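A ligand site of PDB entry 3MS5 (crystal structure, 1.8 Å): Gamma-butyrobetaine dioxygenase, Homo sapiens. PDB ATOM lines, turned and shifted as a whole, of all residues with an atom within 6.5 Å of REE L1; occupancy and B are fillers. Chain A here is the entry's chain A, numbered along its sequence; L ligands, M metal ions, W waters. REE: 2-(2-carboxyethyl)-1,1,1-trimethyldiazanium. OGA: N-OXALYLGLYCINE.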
ATOM      1  N   THR A 176      20.967 -17.994 -20.776  1.00  0.00           N
ATOM      2  CA  THR A 176      22.397 -18.019 -21.029  1.00  0.00           C
ATOM      3  C   THR A 176      23.097 -18.906 -19.959  1.00  0.00           C
ATOM      4  O   THR A 176      22.460 -19.412 -19.044  1.00  0.00           O
ATOM      5  CB  THR A 176      23.039 -16.629 -20.953  1.00  0.00           C
ATOM      6  OG1 THR A 176      23.110 -16.202 -19.595  1.00  0.00           O
ATOM      7  CG2 THR A 176      22.244 -15.552 -21.793  1.00  0.00           C
ATOM      8  N   TYR A 178      24.700 -18.050 -17.480  1.00  0.00           N
ATOM      9  CA  TYR A 178      24.489 -17.490 -16.111  1.00  0.00           C
ATOM     10  C   TYR A 178      23.093 -17.745 -15.552  1.00  0.00           C
ATOM     11  O   TYR A 178      22.821 -17.368 -14.406  1.00  0.00           O
ATOM     12  CB  TYR A 178      24.838 -16.010 -16.066  1.00  0.00           C
ATOM     13  CG  TYR A 178      26.336 -15.791 -16.196  1.00  0.00           C
ATOM     14  CD1 TYR A 178      27.162 -16.011 -15.121  1.00  0.00           C
ATOM     15  CD2 TYR A 178      26.922 -15.467 -17.411  1.00  0.00           C
ATOM     16  CE1 TYR A 178      28.580 -15.847 -15.203  1.00  0.00           C
ATOM     17  CE2 TYR A 178      28.353 -15.330 -17.534  1.00  0.00           C
ATOM     18  CZ  TYR A 178      29.149 -15.511 -16.405  1.00  0.00           C
ATOM     19  OH  TYR A 178      30.521 -15.359 -16.466  1.00  0.00           O
ATOM     20  N   TRP A 182      19.696 -14.223 -12.951  1.00  0.00           N
ATOM     21  CA  TRP A 182      20.976 -14.281 -12.230  1.00  0.00           C
ATOM     22  C   TRP A 182      21.052 -13.284 -11.104  1.00  0.00           C
ATOM     23  O   TRP A 182      20.374 -12.239 -11.115  1.00  0.00           O
ATOM     24  CB  TRP A 182      22.167 -14.123 -13.149  1.00  0.00           C
ATOM     25  CG  TRP A 182      21.919 -13.271 -14.334  1.00  0.00           C
ATOM     26  CD1 TRP A 182      21.541 -13.741 -15.561  1.00  0.00           C
ATOM     27  CD2 TRP A 182      22.039 -11.842 -14.478  1.00  0.00           C
ATOM     28  NE1 TRP A 182      21.389 -12.701 -16.434  1.00  0.00           N
ATOM     29  CE2 TRP A 182      21.683 -11.518 -15.823  1.00  0.00           C
ATOM     30  CE3 TRP A 182      22.396 -10.797 -13.629  1.00  0.00           C
ATOM     31  CZ2 TRP A 182      21.698 -10.224 -16.334  1.00  0.00           C
ATOM     32  CZ3 TRP A 182      22.390  -9.484 -14.130  1.00  0.00           C
ATOM     33  CH2 TRP A 182      22.048  -9.222 -15.487  1.00  0.00           C
ATOM     34  N   VAL A 184      23.069 -10.681  -8.870  1.00  0.00           N
ATOM     35  CA  VAL A 184      24.262  -9.823  -8.738  1.00  0.00           C
ATOM     36  C   VAL A 184      24.471  -9.550  -7.268  1.00  0.00           C
ATOM     37  O   VAL A 184      23.767  -8.740  -6.654  1.00  0.00           O
ATOM     38  CB  VAL A 184      24.100  -8.518  -9.489  1.00  0.00           C
ATOM     39  CG1 VAL A 184      25.441  -7.688  -9.415  1.00  0.00           C
ATOM     40  CG2 VAL A 184      23.654  -8.781 -10.983  1.00  0.00           C
ATOM     41  N   ASN A 191      32.621 -16.156 -10.184  1.00  0.00           N
ATOM     42  CA  ASN A 191      32.925 -16.540 -11.554  1.00  0.00           C
ATOM     43  C   ASN A 191      32.840 -15.384 -12.533  1.00  0.00           C
ATOM     44  O   ASN A 191      33.045 -15.569 -13.749  1.00  0.00           O
ATOM     45  CB  ASN A 191      32.032 -17.716 -12.003  1.00  0.00           C
ATOM     46  CG  ASN A 191      30.563 -17.357 -12.068  1.00  0.00           C
ATOM     47  OD1 ASN A 191      30.212 -16.160 -12.101  1.00  0.00           O
ATOM     48  ND2 ASN A 191      29.702 -18.367 -12.179  1.00  0.00           N
ATOM     49  N   ASN A 192      32.632 -14.176 -12.027  1.00  0.00           N
ATOM     50  CA  ASN A 192      32.483 -12.999 -12.861  1.00  0.00           C
ATOM     51  C   ASN A 192      32.760 -11.755 -12.010  1.00  0.00           C
ATOM     52  O   ASN A 192      32.380 -11.708 -10.852  1.00  0.00           O
ATOM     53  CB  ASN A 192      31.069 -12.958 -13.481  1.00  0.00           C
ATOM     54  CG  ASN A 192      30.942 -11.957 -14.631  1.00  0.00           C
ATOM     55  OD1 ASN A 192      30.868 -10.748 -14.412  1.00  0.00           O
ATOM     56  ND2 ASN A 192      30.876 -12.471 -15.876  1.00  0.00           N
ATOM     57  N   ALA A 194      31.386  -9.145 -11.968  1.00  0.00           N
ATOM     58  CA  ALA A 194      30.094  -8.636 -11.503  1.00  0.00           C
ATOM     59  C   ALA A 194      29.745  -9.066 -10.071  1.00  0.00           C
ATOM     60  O   ALA A 194      29.124  -8.323  -9.317  1.00  0.00           O
ATOM     61  CB  ALA A 194      28.948  -9.070 -12.488  1.00  0.00           C
ATOM     62  N   TYR A 195      30.146 -10.272  -9.717  1.00  0.00           N
ATOM     63  CA  TYR A 195      29.717 -10.913  -8.473  1.00  0.00           C
ATOM     64  C   TYR A 195      30.773 -10.641  -7.373  1.00  0.00           C
ATOM     65  O   TYR A 195      31.151 -11.546  -6.638  1.00  0.00           O
ATOM     66  CB  TYR A 195      29.489 -12.390  -8.699  1.00  0.00           C
ATOM     67  CG  TYR A 195      28.452 -12.743  -9.755  1.00  0.00           C
ATOM     68  CD1 TYR A 195      27.419 -11.856 -10.092  1.00  0.00           C
ATOM     69  CD2 TYR A 195      28.462 -13.981 -10.397  1.00  0.00           C
ATOM     70  CE1 TYR A 195      26.425 -12.190 -11.045  1.00  0.00           C
ATOM     71  CE2 TYR A 195      27.501 -14.293 -11.387  1.00  0.00           C
ATOM     72  CZ  TYR A 195      26.467 -13.391 -11.651  1.00  0.00           C
ATOM     73  OH  TYR A 195      25.479 -13.675 -12.564  1.00  0.00           O
ATOM     74  N   HIS A 203      30.386  -1.051 -19.562  1.00  0.00           N
ATOM     75  CA  HIS A 203      30.414  -2.261 -20.351  1.00  0.00           C
ATOM     76  C   HIS A 203      29.031  -2.482 -20.950  1.00  0.00           C
ATOM     77  O   HIS A 203      28.023  -1.906 -20.483  1.00  0.00           O
ATOM     78  CB  HIS A 203      30.813  -3.477 -19.535  1.00  0.00           C
ATOM     79  CG  HIS A 203      29.858  -3.823 -18.456  1.00  0.00           C
ATOM     80  ND1 HIS A 203      29.821  -3.161 -17.254  1.00  0.00           N
ATOM     81  CD2 HIS A 203      28.895  -4.785 -18.382  1.00  0.00           C
ATOM     82  CE1 HIS A 203      28.876  -3.691 -16.492  1.00  0.00           C
ATOM     83  NE2 HIS A 203      28.287  -4.663 -17.164  1.00  0.00           N
ATOM     84  N   THR A 204      29.013  -3.273 -22.013  1.00  0.00           N
ATOM     85  CA  THR A 204      27.841  -4.019 -22.463  1.00  0.00           C
ATOM     86  C   THR A 204      27.940  -5.444 -21.889  1.00  0.00           C
ATOM     87  O   THR A 204      29.014  -5.946 -21.630  1.00  0.00           O
ATOM     88  CB  THR A 204      27.723  -4.031 -24.007  1.00  0.00           C
ATOM     89  OG1 THR A 204      28.819  -4.739 -24.593  1.00  0.00           O
ATOM     90  CG2 THR A 204      27.662  -2.623 -24.602  1.00  0.00           C
ATOM     91  N   ASP A 205      26.789  -6.096 -21.622  1.00  0.00           N
ATOM     92  CA  ASP A 205      26.821  -7.449 -21.128  1.00  0.00           C
ATOM     93  C   ASP A 205      27.005  -8.426 -22.242  1.00  0.00           C
ATOM     94  O   ASP A 205      26.379  -8.348 -23.290  1.00  0.00           O
ATOM     95  CB  ASP A 205      25.573  -7.822 -20.379  1.00  0.00           C
ATOM     96  CG  ASP A 205      25.624  -7.451 -18.921  1.00  0.00           C
ATOM     97  OD1 ASP A 205      26.332  -6.507 -18.530  1.00  0.00           O
ATOM     98  OD2 ASP A 205      24.916  -8.129 -18.133  1.00  0.00           O
ATOM     99  N   TYR A 206      27.897  -9.364 -21.998  1.00  0.00           N
ATOM    100  CA  TYR A 206      28.015 -10.593 -22.749  1.00  0.00           C
ATOM    101  C   TYR A 206      28.563 -10.532 -24.174  1.00  0.00           C
ATOM    102  O   TYR A 206      28.153 -11.300 -25.017  1.00  0.00           O
ATOM    103  CB  TYR A 206      26.709 -11.445 -22.669  1.00  0.00           C
ATOM    104  CG  TYR A 206      26.810 -12.842 -22.048  1.00  0.00           C
ATOM    105  CD1 TYR A 206      25.755 -13.352 -21.300  1.00  0.00           C
ATOM    106  CD2 TYR A 206      27.937 -13.654 -22.236  1.00  0.00           C
ATOM    107  CE1 TYR A 206      25.813 -14.629 -20.786  1.00  0.00           C
ATOM    108  CE2 TYR A 206      27.971 -14.929 -21.739  1.00  0.00           C
ATOM    109  CZ  TYR A 206      26.913 -15.386 -20.964  1.00  0.00           C
ATOM    110  OH  TYR A 206      26.926 -16.670 -20.463  1.00  0.00           O
ATOM    111  N   PRO A 207      29.576  -9.654 -24.446  1.00  0.00           N
ATOM    112  CA  PRO A 207      30.208  -9.713 -25.757  1.00  0.00           C
ATOM    113  C   PRO A 207      30.952 -11.045 -26.007  1.00  0.00           C
ATOM    114  O   PRO A 207      31.363 -11.302 -27.117  1.00  0.00           O
ATOM    115  CB  PRO A 207      31.163  -8.508 -25.750  1.00  0.00           C
ATOM    116  CG  PRO A 207      31.489  -8.339 -24.239  1.00  0.00           C
ATOM    117  CD  PRO A 207      30.149  -8.593 -23.598  1.00  0.00           C
ATOM    118  N   ALA A 208      31.160 -11.868 -24.981  1.00  0.00           N
ATOM    119  CA  ALA A 208      31.668 -13.250 -25.160  1.00  0.00           C
ATOM    120  C   ALA A 208      30.730 -14.123 -25.997  1.00  0.00           C
ATOM    121  O   ALA A 208      31.116 -15.182 -26.456  1.00  0.00           O
ATOM    122  CB  ALA A 208      32.002 -13.942 -23.773  1.00  0.00           C
ATOM    123  N   GLN A 216      18.340  -5.970 -21.481  1.00  0.00           N
ATOM    124  CA  GLN A 216      18.649  -6.368 -20.133  1.00  0.00           C
ATOM    125  C   GLN A 216      17.568  -5.912 -19.171  1.00  0.00           C
ATOM    126  O   GLN A 216      17.093  -4.801 -19.262  1.00  0.00           O
ATOM    127  CB  GLN A 216      19.996  -5.722 -19.735  1.00  0.00           C
ATOM    128  CG  GLN A 216      20.580  -6.344 -18.557  1.00  0.00           C
ATOM    129  CD  GLN A 216      21.912  -5.759 -18.141  1.00  0.00           C
ATOM    130  OE1 GLN A 216      22.075  -5.549 -16.989  1.00  0.00           O
ATOM    131  NE2 GLN A 216      22.870  -5.553 -19.089  1.00  0.00           N
ATOM    132  N   LEU A 218      17.021  -5.462 -14.945  1.00  0.00           N
ATOM    133  CA  LEU A 218      17.761  -5.501 -13.666  1.00  0.00           C
ATOM    134  C   LEU A 218      16.888  -4.965 -12.558  1.00  0.00           C
ATOM    135  O   LEU A 218      16.460  -3.818 -12.607  1.00  0.00           O
ATOM    136  CB  LEU A 218      19.067  -4.673 -13.698  1.00  0.00           C
ATOM    137  CG  LEU A 218      20.377  -5.156 -14.293  1.00  0.00           C
ATOM    138  CD1 LEU A 218      21.458  -4.009 -14.148  1.00  0.00           C
ATOM    139  CD2 LEU A 218      20.854  -6.434 -13.664  1.00  0.00           C
ATOM    140  N   ASP A 262      35.017 -16.292 -21.873  1.00  0.00           N
ATOM    141  CA  ASP A 262      34.451 -16.506 -20.549  1.00  0.00           C
ATOM    142  C   ASP A 262      34.563 -17.995 -20.239  1.00  0.00           C
ATOM    143  O   ASP A 262      34.076 -18.829 -21.013  1.00  0.00           O
ATOM    144  CB  ASP A 262      32.987 -16.082 -20.501  1.00  0.00           C
ATOM    145  CG  ASP A 262      32.462 -15.836 -19.094  1.00  0.00           C
ATOM    146  OD1 ASP A 262      33.277 -15.660 -18.138  1.00  0.00           O
ATOM    147  OD2 ASP A 262      31.232 -15.745 -18.962  1.00  0.00           O
ATOM    148  N   ASN A 293      33.167  -5.311 -23.049  1.00  0.00           N
ATOM    149  CA  ASN A 293      33.286  -5.541 -21.599  1.00  0.00           C
ATOM    150  C   ASN A 293      34.776  -5.742 -21.339  1.00  0.00           C
ATOM    151  O   ASN A 293      35.405  -6.700 -21.829  1.00  0.00           O
ATOM    152  CB  ASN A 293      32.456  -6.725 -21.167  1.00  0.00           C
ATOM    153  CG  ASN A 293      32.577  -7.051 -19.665  1.00  0.00           C
ATOM    154  OD1 ASN A 293      33.424  -6.469 -18.942  1.00  0.00           O
ATOM    155  ND2 ASN A 293      31.752  -8.002 -19.206  1.00  0.00           N
ATOM    156  N   THR A 296      36.041  -9.143 -19.899  1.00  0.00           N
ATOM    157  CA  THR A 296      36.016 -10.374 -20.699  1.00  0.00           C
ATOM    158  C   THR A 296      36.738 -10.308 -22.010  1.00  0.00           C
ATOM    159  O   THR A 296      36.922 -11.315 -22.701  1.00  0.00           O
ATOM    160  CB  THR A 296      34.569 -10.874 -20.940  1.00  0.00           C
ATOM    161  OG1 THR A 296      33.851  -9.919 -21.733  1.00  0.00           O
ATOM    162  CG2 THR A 296      33.848 -11.118 -19.564  1.00  0.00           C
ATOM    163  N   HIS A 348      26.783   0.443 -19.425  1.00  0.00           N
ATOM    164  CA  HIS A 348      26.335   0.608 -18.033  1.00  0.00           C
ATOM    165  C   HIS A 348      27.427   0.155 -17.089  1.00  0.00           C
ATOM    166  O   HIS A 348      28.399  -0.568 -17.467  1.00  0.00           O
ATOM    167  CB  HIS A 348      25.049  -0.161 -17.778  1.00  0.00           C
ATOM    168  CG  HIS A 348      25.212  -1.657 -17.916  1.00  0.00           C
ATOM    169  ND1 HIS A 348      25.382  -2.277 -19.126  1.00  0.00           N
ATOM    170  CD2 HIS A 348      25.328  -2.625 -16.971  1.00  0.00           C
ATOM    171  CE1 HIS A 348      25.580  -3.582 -18.934  1.00  0.00           C
ATOM    172  NE2 HIS A 348      25.566  -3.824 -17.628  1.00  0.00           N
ATOM    173  N   TYR A 367      17.873 -11.386 -19.340  1.00  0.00           N
ATOM    174  CA  TYR A 367      17.982 -10.893 -20.697  1.00  0.00           C
ATOM    175  C   TYR A 367      16.771 -11.262 -21.546  1.00  0.00           C
ATOM    176  O   TYR A 367      16.122 -12.294 -21.313  1.00  0.00           O
ATOM    177  CB  TYR A 367      19.230 -11.482 -21.353  1.00  0.00           C
ATOM    178  CG  TYR A 367      20.565 -11.220 -20.636  1.00  0.00           C
ATOM    179  CD1 TYR A 367      21.053  -9.929 -20.450  1.00  0.00           C
ATOM    180  CD2 TYR A 367      21.364 -12.278 -20.197  1.00  0.00           C
ATOM    181  CE1 TYR A 367      22.246  -9.695 -19.803  1.00  0.00           C
ATOM    182  CE2 TYR A 367      22.612 -12.072 -19.585  1.00  0.00           C
ATOM    183  CZ  TYR A 367      23.059 -10.766 -19.402  1.00  0.00           C
ATOM    184  OH  TYR A 367      24.260 -10.548 -18.747  1.00  0.00           O
HETATM  185  C1  REE L   1      29.504 -10.288 -18.989  1.00  0.00           C
HETATM  186  N1  REE L   1      27.015 -10.965 -16.943  1.00  0.00           N
HETATM  187  O1  REE L   1      30.057 -11.231 -18.401  1.00  0.00           O
HETATM  188  C2  REE L   1      28.468  -9.449 -18.248  1.00  0.00           C
HETATM  189  N2  REE L   1      26.400 -11.395 -15.707  1.00  0.00           N
HETATM  190  O2  REE L   1      29.848  -9.817 -20.113  1.00  0.00           O
HETATM  191  C3  REE L   1      27.994  -9.896 -16.861  1.00  0.00           C
HETATM  192  C4  REE L   1      25.370 -12.385 -16.098  1.00  0.00           C
HETATM  193  C5  REE L   1      27.396 -12.106 -14.861  1.00  0.00           C
HETATM  194  C6  REE L   1      25.828 -10.286 -14.935  1.00  0.00           C
HETATM  195  C1  OGA L   2      26.565  -6.727 -14.285  1.00  0.00           C
HETATM  196  C2  OGA L   2      26.136  -5.298 -13.961  1.00  0.00           C
HETATM  197  C4  OGA L   2      25.356  -3.601 -12.385  1.00  0.00           C
HETATM  198  C5  OGA L   2      25.204  -3.429 -10.860  1.00  0.00           C
HETATM  199  O1  OGA L   2      26.347  -7.561 -13.388  1.00  0.00           O
HETATM  200  O2  OGA L   2      26.985  -6.975 -15.434  1.00  0.00           O
HETATM  201  O2' OGA L   2      26.252  -4.465 -14.830  1.00  0.00           O
HETATM  202  O3  OGA L   2      25.647  -4.323 -10.099  1.00  0.00           O
HETATM  203  N1  OGA L   2      25.694  -5.001 -12.726  1.00  0.00           N
HETATM  204  O4  OGA L   2      24.635  -2.377 -10.510  1.00  0.00           O
HETATM  205 NI    NI M   1      26.401  -5.443 -16.662  1.00  0.00          NI
HETATM  206  O   HOH W   1      30.845 -13.115 -20.049  1.00  0.00           O
HETATM  207  O   HOH W   2      31.353 -11.322 -21.960  1.00  0.00           O
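CG of Tyr 178 touches C4 of REE L1, at 3.5 Å. Trp 182 touches REE L1. OH of Tyr 195 touches C5 of REE L1 (3.4 Å). CG of Asp 205 touches C2 of REE L1, at 3.5 Å. CD of Pro 207 touches O2 of REE L1, 3.7 Å away. CG2 of Thr 296 touches O1 of REE L1 (3.97 Å). Hydrophobic or aromatic side chains that line REE L1: Tyr 178, Trp 182, Tyr 195 and Pro 207. Ten residues have an atom within 4 Å of REE L1: Tyr 178, Trp 182, Asn 192, Tyr 195, Asp 205, Tyr 206, Pro 207, Asn 293, Thr 296 and Tyr 367. Along chain A the residues within 4 Å of REE L1 span positions 178 to 367. The nearest printed residue that does not touch REE L1 is Ala 194 (4.1 Å).
The backbone NH (N) of Tyr 206 sits at hydrogen-bond distance from an oxygen (O2) of REE L1. An oxygen (O2) of REE L1 lies within hydrogen-bond range of the side-chain amide nitrogen (ND2) of Asn 293, 2.8 Å away. The side-chain amide nitrogen of Asn 192 sits at hydrogen-bond distance from an oxygen (O1) of REE L1. A nitrogen (N1) of REE L1 is in hydrogen-bond range of the side-chain hydroxyl (OH) of Tyr 367 (3.3 Å).
ND2 of Asn 192 sits at hydrogen-bond distance from OH of Tyr 178, at 3.0 Å. OD1 of Asn 192 lies close to N of Ala 194 (3.0 Å). OD2 of Asp 205 sits at hydrogen-bond distance from OH of Tyr 367 (2.6 Å). OD2 of Asp 205 sits close to NE2 of Gln 216. OD2 of Asp 262 sits at hydrogen-bond distance from OH of Tyr 178 (2.6 Å). N of Tyr 178 sits close to OG1 of Thr 176, 3.2 Å away.
Water W1 lies within hydrogen-bond range of an oxygen (O1) of REE L1 (2.6 Å) and the side-chain carboxylate of Asp 262 (2.9 Å). Water W2 lies within hydrogen-bond range of O2 of REE L1 (2.8 Å), OG1 of Thr 296 (2.9 Å) and N of Ala 208 (3.1 Å).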
